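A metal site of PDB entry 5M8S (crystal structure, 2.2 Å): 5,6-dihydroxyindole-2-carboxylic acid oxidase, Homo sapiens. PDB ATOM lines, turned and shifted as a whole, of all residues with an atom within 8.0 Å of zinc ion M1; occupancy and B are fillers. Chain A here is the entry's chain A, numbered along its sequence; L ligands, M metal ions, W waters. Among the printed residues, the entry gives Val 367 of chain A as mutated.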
ATOM      1  N   HIS A 168       1.505  -9.548 -31.036  1.00  0.00           N
ATOM      2  CA  HIS A 168       2.567  -9.265 -30.075  1.00  0.00           C
ATOM      3  C   HIS A 168       2.027  -8.407 -28.942  1.00  0.00           C
ATOM      4  O   HIS A 168       2.258  -8.698 -27.757  1.00  0.00           O
ATOM      5  CB  HIS A 168       3.725  -8.556 -30.783  1.00  0.00           C
ATOM      6  CG  HIS A 168       5.032  -8.540 -30.033  1.00  0.00           C
ATOM      7  ND1 HIS A 168       5.398  -7.504 -29.180  1.00  0.00           N
ATOM      8  CD2 HIS A 168       6.074  -9.401 -30.047  1.00  0.00           C
ATOM      9  CE1 HIS A 168       6.613  -7.748 -28.712  1.00  0.00           C
ATOM     10  NE2 HIS A 168       7.048  -8.887 -29.224  1.00  0.00           N
ATOM     11  N   TYR A 169       1.259  -7.365 -29.283  1.00  0.00           N
ATOM     12  CA  TYR A 169       0.670  -6.513 -28.255  1.00  0.00           C
ATOM     13  C   TYR A 169      -0.212  -7.341 -27.338  1.00  0.00           C
ATOM     14  O   TYR A 169      -0.135  -7.225 -26.111  1.00  0.00           O
ATOM     15  CB  TYR A 169      -0.123  -5.355 -28.877  1.00  0.00           C
ATOM     16  CG  TYR A 169      -1.298  -4.943 -27.995  1.00  0.00           C
ATOM     17  CD1 TYR A 169      -1.126  -4.041 -26.949  1.00  0.00           C
ATOM     18  CD2 TYR A 169      -2.569  -5.494 -28.192  1.00  0.00           C
ATOM     19  CE1 TYR A 169      -2.192  -3.698 -26.111  1.00  0.00           C
ATOM     20  CE2 TYR A 169      -3.637  -5.146 -27.371  1.00  0.00           C
ATOM     21  CZ  TYR A 169      -3.445  -4.241 -26.338  1.00  0.00           C
ATOM     22  OH  TYR A 169      -4.533  -3.929 -25.530  1.00  0.00           O
ATOM     23  N   SER A 171      -0.032 -10.416 -26.619  1.00  0.00           N
ATOM     24  CA  SER A 171       0.689 -11.330 -25.759  1.00  0.00           C
ATOM     25  C   SER A 171       1.342 -10.606 -24.583  1.00  0.00           C
ATOM     26  O   SER A 171       1.670 -11.276 -23.594  1.00  0.00           O
ATOM     27  CB  SER A 171       1.767 -12.100 -26.552  1.00  0.00           C
ATOM     28  OG  SER A 171       2.883 -11.262 -26.820  1.00  0.00           O
ATOM     29  N   VAL A 172       1.515  -9.282 -24.650  1.00  0.00           N
ATOM     30  CA  VAL A 172       2.185  -8.564 -23.567  1.00  0.00           C
ATOM     31  C   VAL A 172       1.259  -7.680 -22.759  1.00  0.00           C
ATOM     32  O   VAL A 172       1.684  -7.182 -21.702  1.00  0.00           O
ATOM     33  CB  VAL A 172       3.367  -7.706 -24.092  1.00  0.00           C
ATOM     34  CG1 VAL A 172       4.337  -8.558 -24.920  1.00  0.00           C
ATOM     35  CG2 VAL A 172       2.833  -6.487 -24.888  1.00  0.00           C
ATOM     36  N   ASP A 188       3.580 -11.902 -18.950  1.00  0.00           N
ATOM     37  CA  ASP A 188       4.074 -11.663 -20.317  1.00  0.00           C
ATOM     38  C   ASP A 188       4.118 -13.004 -21.024  1.00  0.00           C
ATOM     39  O   ASP A 188       4.925 -13.864 -20.654  1.00  0.00           O
ATOM     40  CB  ASP A 188       5.441 -10.984 -20.294  1.00  0.00           C
ATOM     41  CG  ASP A 188       5.890 -10.461 -21.666  1.00  0.00           C
ATOM     42  OD1 ASP A 188       5.532 -11.091 -22.689  1.00  0.00           O
ATOM     43  OD2 ASP A 188       6.645  -9.450 -21.705  1.00  0.00           O
ATOM     44  N   SER A 190       5.087 -13.856 -23.975  1.00  0.00           N
ATOM     45  CA  SER A 190       6.089 -14.046 -25.033  1.00  0.00           C
ATOM     46  C   SER A 190       7.480 -13.565 -24.665  1.00  0.00           C
ATOM     47  O   SER A 190       8.395 -13.670 -25.504  1.00  0.00           O
ATOM     48  CB  SER A 190       5.634 -13.323 -26.314  1.00  0.00           C
ATOM     49  OG  SER A 190       5.327 -11.973 -26.029  1.00  0.00           O
ATOM     50  N   HIS A 191       7.690 -13.033 -23.457  1.00  0.00           N
ATOM     51  CA  HIS A 191       8.995 -12.559 -23.018  1.00  0.00           C
ATOM     52  C   HIS A 191       9.211 -12.974 -21.582  1.00  0.00           C
ATOM     53  O   HIS A 191       8.279 -13.404 -20.890  1.00  0.00           O
ATOM     54  CB  HIS A 191       9.123 -11.040 -23.118  1.00  0.00           C
ATOM     55  CG  HIS A 191       8.746 -10.507 -24.452  1.00  0.00           C
ATOM     56  ND1 HIS A 191       7.434 -10.309 -24.839  1.00  0.00           N
ATOM     57  CD2 HIS A 191       9.502 -10.205 -25.541  1.00  0.00           C
ATOM     58  CE1 HIS A 191       7.404  -9.849 -26.078  1.00  0.00           C
ATOM     59  NE2 HIS A 191       8.645  -9.773 -26.519  1.00  0.00           N
ATOM     60  N   PHE A 196      10.112 -17.286 -25.013  1.00  0.00           N
ATOM     61  CA  PHE A 196      10.523 -16.103 -25.780  1.00  0.00           C
ATOM     62  C   PHE A 196      10.973 -16.494 -27.190  1.00  0.00           C
ATOM     63  O   PHE A 196      10.530 -15.889 -28.173  1.00  0.00           O
ATOM     64  CB  PHE A 196      11.638 -15.359 -25.033  1.00  0.00           C
ATOM     65  CG  PHE A 196      12.378 -14.359 -25.872  1.00  0.00           C
ATOM     66  CD1 PHE A 196      11.779 -13.159 -26.220  1.00  0.00           C
ATOM     67  CD2 PHE A 196      13.671 -14.615 -26.321  1.00  0.00           C
ATOM     68  CE1 PHE A 196      12.462 -12.206 -27.000  1.00  0.00           C
ATOM     69  CE2 PHE A 196      14.360 -13.675 -27.105  1.00  0.00           C
ATOM     70  CZ  PHE A 196      13.750 -12.467 -27.438  1.00  0.00           C
ATOM     71  N   TRP A 199       8.073 -18.442 -29.300  1.00  0.00           N
ATOM     72  CA  TRP A 199       6.982 -17.527 -29.638  1.00  0.00           C
ATOM     73  C   TRP A 199       7.362 -16.660 -30.843  1.00  0.00           C
ATOM     74  O   TRP A 199       6.638 -16.594 -31.844  1.00  0.00           O
ATOM     75  CB  TRP A 199       6.631 -16.660 -28.425  1.00  0.00           C
ATOM     76  CG  TRP A 199       5.338 -15.903 -28.552  1.00  0.00           C
ATOM     77  CD1 TRP A 199       4.151 -16.204 -27.962  1.00  0.00           C
ATOM     78  CD2 TRP A 199       5.108 -14.726 -29.342  1.00  0.00           C
ATOM     79  NE1 TRP A 199       3.186 -15.290 -28.336  1.00  0.00           N
ATOM     80  CE2 TRP A 199       3.750 -14.368 -29.185  1.00  0.00           C
ATOM     81  CE3 TRP A 199       5.911 -13.923 -30.176  1.00  0.00           C
ATOM     82  CZ2 TRP A 199       3.171 -13.258 -29.830  1.00  0.00           C
ATOM     83  CZ3 TRP A 199       5.340 -12.811 -30.815  1.00  0.00           C
ATOM     84  CH2 TRP A 199       3.992 -12.501 -30.641  1.00  0.00           C
ATOM     85  N   HIS A 200       8.524 -16.010 -30.767  1.00  0.00           N
ATOM     86  CA  HIS A 200       8.931 -15.105 -31.846  1.00  0.00           C
ATOM     87  C   HIS A 200       9.260 -15.863 -33.115  1.00  0.00           C
ATOM     88  O   HIS A 200       9.089 -15.335 -34.211  1.00  0.00           O
ATOM     89  CB  HIS A 200      10.098 -14.244 -31.385  1.00  0.00           C
ATOM     90  CG  HIS A 200       9.707 -13.219 -30.373  1.00  0.00           C
ATOM     91  ND1 HIS A 200       9.508 -13.530 -29.048  1.00  0.00           N
ATOM     92  CD2 HIS A 200       9.458 -11.897 -30.494  1.00  0.00           C
ATOM     93  CE1 HIS A 200       9.141 -12.444 -28.388  1.00  0.00           C
ATOM     94  NE2 HIS A 200       9.106 -11.437 -29.242  1.00  0.00           N
ATOM     95  N   HIS A 203       5.870 -16.272 -34.669  1.00  0.00           N
ATOM     96  CA  HIS A 203       5.534 -14.912 -35.084  1.00  0.00           C
ATOM     97  C   HIS A 203       6.135 -14.600 -36.467  1.00  0.00           C
ATOM     98  O   HIS A 203       5.416 -14.161 -37.377  1.00  0.00           O
ATOM     99  CB  HIS A 203       6.032 -13.947 -34.009  1.00  0.00           C
ATOM    100  CG  HIS A 203       5.453 -12.556 -34.073  1.00  0.00           C
ATOM    101  ND1 HIS A 203       6.189 -11.435 -33.767  1.00  0.00           N
ATOM    102  CD2 HIS A 203       4.199 -12.117 -34.334  1.00  0.00           C
ATOM    103  CE1 HIS A 203       5.431 -10.361 -33.869  1.00  0.00           C
ATOM    104  NE2 HIS A 203       4.219 -10.741 -34.221  1.00  0.00           N
ATOM    105  N   GLU A 336      18.048 -13.302 -24.923  1.00  0.00           N
ATOM    106  CA  GLU A 336      16.998 -12.300 -24.749  1.00  0.00           C
ATOM    107  C   GLU A 336      17.593 -10.982 -24.252  1.00  0.00           C
ATOM    108  O   GLU A 336      17.167  -9.897 -24.666  1.00  0.00           O
ATOM    109  CB  GLU A 336      15.910 -12.800 -23.781  1.00  0.00           C
ATOM    110  CG  GLU A 336      14.726 -11.803 -23.645  1.00  0.00           C
ATOM    111  CD  GLU A 336      13.485 -12.384 -22.928  1.00  0.00           C
ATOM    112  OE1 GLU A 336      13.568 -13.517 -22.400  1.00  0.00           O
ATOM    113  OE2 GLU A 336      12.433 -11.703 -22.879  1.00  0.00           O
ATOM    114  N   HIS A 353      19.480  -9.057 -27.661  1.00  0.00           N
ATOM    115  CA  HIS A 353      18.150  -8.691 -28.143  1.00  0.00           C
ATOM    116  C   HIS A 353      17.583  -7.486 -27.412  1.00  0.00           C
ATOM    117  O   HIS A 353      17.087  -6.536 -28.038  1.00  0.00           O
ATOM    118  CB  HIS A 353      17.216  -9.895 -28.022  1.00  0.00           C
ATOM    119  CG  HIS A 353      15.755  -9.541 -27.946  1.00  0.00           C
ATOM    120  ND1 HIS A 353      15.101  -9.332 -26.754  1.00  0.00           N
ATOM    121  CD2 HIS A 353      14.816  -9.446 -28.916  1.00  0.00           C
ATOM    122  CE1 HIS A 353      13.829  -9.074 -26.986  1.00  0.00           C
ATOM    123  NE2 HIS A 353      13.635  -9.128 -28.295  1.00  0.00           N
ATOM    124  N   ASN A 354      17.643  -7.496 -26.072  1.00  0.00           N
ATOM    125  CA  ASN A 354      17.098  -6.364 -25.331  1.00  0.00           C
ATOM    126  C   ASN A 354      17.858  -5.076 -25.673  1.00  0.00           C
ATOM    127  O   ASN A 354      17.241  -4.019 -25.845  1.00  0.00           O
ATOM    128  CB  ASN A 354      17.111  -6.629 -23.828  1.00  0.00           C
ATOM    129  CG  ASN A 354      15.964  -7.549 -23.369  1.00  0.00           C
ATOM    130  OD1 ASN A 354      15.031  -7.843 -24.124  1.00  0.00           O
ATOM    131  ND2 ASN A 354      16.006  -7.984 -22.120  1.00  0.00           N
ATOM    132  N   HIS A 357      16.905  -3.629 -29.090  1.00  0.00           N
ATOM    133  CA  HIS A 357      15.651  -2.912 -28.962  1.00  0.00           C
ATOM    134  C   HIS A 357      15.864  -1.527 -28.368  1.00  0.00           C
ATOM    135  O   HIS A 357      15.391  -0.517 -28.922  1.00  0.00           O
ATOM    136  CB  HIS A 357      14.668  -3.697 -28.091  1.00  0.00           C
ATOM    137  CG  HIS A 357      13.799  -4.673 -28.832  1.00  0.00           C
ATOM    138  ND1 HIS A 357      12.790  -4.271 -29.673  1.00  0.00           N
ATOM    139  CD2 HIS A 357      13.724  -6.017 -28.772  1.00  0.00           C
ATOM    140  CE1 HIS A 357      12.150  -5.332 -30.133  1.00  0.00           C
ATOM    141  NE2 HIS A 357      12.706  -6.403 -29.607  1.00  0.00           N
ATOM    142  N   VAL A 367       7.799  -1.694 -25.226  1.00  0.00           N
ATOM    143  CA  VAL A 367       7.308  -3.070 -25.132  1.00  0.00           C
ATOM    144  C   VAL A 367       5.914  -3.212 -25.756  1.00  0.00           C
ATOM    145  O   VAL A 367       5.593  -4.272 -26.315  1.00  0.00           O
ATOM    146  CB  VAL A 367       7.349  -3.585 -23.681  1.00  0.00           C
ATOM    147  CG1 VAL A 367       8.774  -3.611 -23.172  1.00  0.00           C
ATOM    148  CG2 VAL A 367       6.462  -2.746 -22.738  1.00  0.00           C
ATOM    149  N   SER A 370       6.804  -2.245 -30.099  1.00  0.00           N
ATOM    150  CA  SER A 370       8.022  -2.465 -30.872  1.00  0.00           C
ATOM    151  C   SER A 370       7.807  -3.013 -32.282  1.00  0.00           C
ATOM    152  O   SER A 370       8.485  -2.516 -33.197  1.00  0.00           O
ATOM    153  CB  SER A 370       8.987  -3.328 -30.057  1.00  0.00           C
ATOM    154  OG  SER A 370       8.421  -4.575 -29.633  1.00  0.00           O
ATOM    155  N   PRO A 371       6.875  -3.946 -32.560  1.00  0.00           N
ATOM    156  CA  PRO A 371       6.729  -4.416 -33.950  1.00  0.00           C
ATOM    157  C   PRO A 371       6.245  -3.344 -34.911  1.00  0.00           C
ATOM    158  O   PRO A 371       6.322  -3.556 -36.132  1.00  0.00           O
ATOM    159  CB  PRO A 371       5.696  -5.536 -33.854  1.00  0.00           C
ATOM    160  CG  PRO A 371       5.639  -5.907 -32.413  1.00  0.00           C
ATOM    161  CD  PRO A 371       5.926  -4.642 -31.676  1.00  0.00           C
ATOM    162  N   PHE A 376      11.933  -4.359 -36.252  1.00  0.00           N
ATOM    163  CA  PHE A 376      11.584  -5.506 -35.410  1.00  0.00           C
ATOM    164  C   PHE A 376      11.710  -6.817 -36.188  1.00  0.00           C
ATOM    165  O   PHE A 376      12.242  -7.797 -35.656  1.00  0.00           O
ATOM    166  CB  PHE A 376      10.147  -5.334 -34.875  1.00  0.00           C
ATOM    167  CG  PHE A 376       9.658  -6.483 -34.009  1.00  0.00           C
ATOM    168  CD1 PHE A 376       9.180  -7.653 -34.576  1.00  0.00           C
ATOM    169  CD2 PHE A 376       9.597  -6.339 -32.633  1.00  0.00           C
ATOM    170  CE1 PHE A 376       8.715  -8.688 -33.798  1.00  0.00           C
ATOM    171  CE2 PHE A 376       9.107  -7.365 -31.839  1.00  0.00           C
ATOM    172  CZ  PHE A 376       8.683  -8.547 -32.425  1.00  0.00           C
ATOM    173  N   LEU A 379      15.411  -7.603 -36.658  1.00  0.00           N
ATOM    174  CA  LEU A 379      15.982  -7.867 -35.346  1.00  0.00           C
ATOM    175  C   LEU A 379      15.651  -9.279 -34.887  1.00  0.00           C
ATOM    176  O   LEU A 379      16.494  -9.975 -34.318  1.00  0.00           O
ATOM    177  CB  LEU A 379      15.455  -6.820 -34.359  1.00  0.00           C
ATOM    178  CG  LEU A 379      16.014  -6.693 -32.940  1.00  0.00           C
ATOM    179  CD1 LEU A 379      15.655  -5.332 -32.374  1.00  0.00           C
ATOM    180  CD2 LEU A 379      15.460  -7.804 -31.994  1.00  0.00           C
ATOM    181  N   HIS A 380      14.436  -9.751 -35.171  1.00  0.00           N
ATOM    182  CA  HIS A 380      14.053 -11.059 -34.652  1.00  0.00           C
ATOM    183  C   HIS A 380      14.371 -12.222 -35.590  1.00  0.00           C
ATOM    184  O   HIS A 380      14.493 -13.352 -35.101  1.00  0.00           O
ATOM    185  CB  HIS A 380      12.573 -11.103 -34.255  1.00  0.00           C
ATOM    186  CG  HIS A 380      12.351 -10.673 -32.843  1.00  0.00           C
ATOM    187  ND1 HIS A 380      12.650 -11.491 -31.768  1.00  0.00           N
ATOM    188  CD2 HIS A 380      11.965  -9.492 -32.325  1.00  0.00           C
ATOM    189  CE1 HIS A 380      12.399 -10.832 -30.649  1.00  0.00           C
ATOM    190  NE2 HIS A 380      11.984  -9.629 -30.958  1.00  0.00           N
HETATM  191  N1  LIG L   1      12.253  -4.605 -24.723  1.00  0.00           N
HETATM  192  N2  LIG L   1      12.124  -2.241 -24.576  1.00  0.00           N
HETATM  193  C1  LIG L   1      12.959  -5.351 -21.065  1.00  0.00           C
HETATM  194  C2  LIG L   1      12.273  -5.235 -22.415  1.00  0.00           C
HETATM  195  C3  LIG L   1      12.906  -4.711 -23.433  1.00  0.00           C
HETATM  196  C4  LIG L   1      14.320  -4.195 -23.268  1.00  0.00           C
HETATM  197  C5  LIG L   1      14.924  -4.276 -22.112  1.00  0.00           C
HETATM  198  C6  LIG L   1      14.190  -4.901 -20.936  1.00  0.00           C
HETATM  199  C7  LIG L   1      11.891  -3.297 -25.243  1.00  0.00           C
HETATM  200  S1  LIG L   1      11.183  -3.222 -26.672  1.00  0.00           S
HETATM  201 ZN    ZN M   1       8.837  -9.494 -28.560  1.00  0.00          ZN
HETATM  202 ZN    ZN M   2      12.079  -8.332 -29.434  1.00  0.00          ZN
HETATM  203  O   HOH W   1      10.222  -8.040 -28.623  1.00  0.00           O
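A ring nitrogen (ND1) of His 357 lies close to a sulfur (S1) of the ligand (3.6 Å).
Merely in contact with zinc ion M1: Phe 376 (3.9 Å) and His 380 (3.96 Å). Within 4 Å of zinc ion M1: His 168, His 191, His 200, Phe 376 and His 380.
A ring nitrogen (ND1) of His 191 sits at hydrogen-bond distance from the side-chain hydroxyl (OG) of Ser 190, 2.9 Å away. The backbone carbonyl oxygen (O) of Phe 196 sits at hydrogen-bond distance from a ring nitrogen (ND1) of His 200. ND1 of His 191 sits at hydrogen-bond distance from OD1 of Asp 188 (3.0 Å). O of His 168 is in hydrogen-bond range of OG of Ser 171 (2.8 Å).
NE2 of His 168 binds zinc ion M1, 2.0 Å away. Water W1 binds zinc ion M1, at 2.0 Å. A ring nitrogen (NE2) of His 191 is bound to zinc ion M1 (2.1 Å). A ring nitrogen (NE2) of His 200 binds zinc ion M1, 2.1 Å away. Zinc ion M1 has four donor atoms within binding distance.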
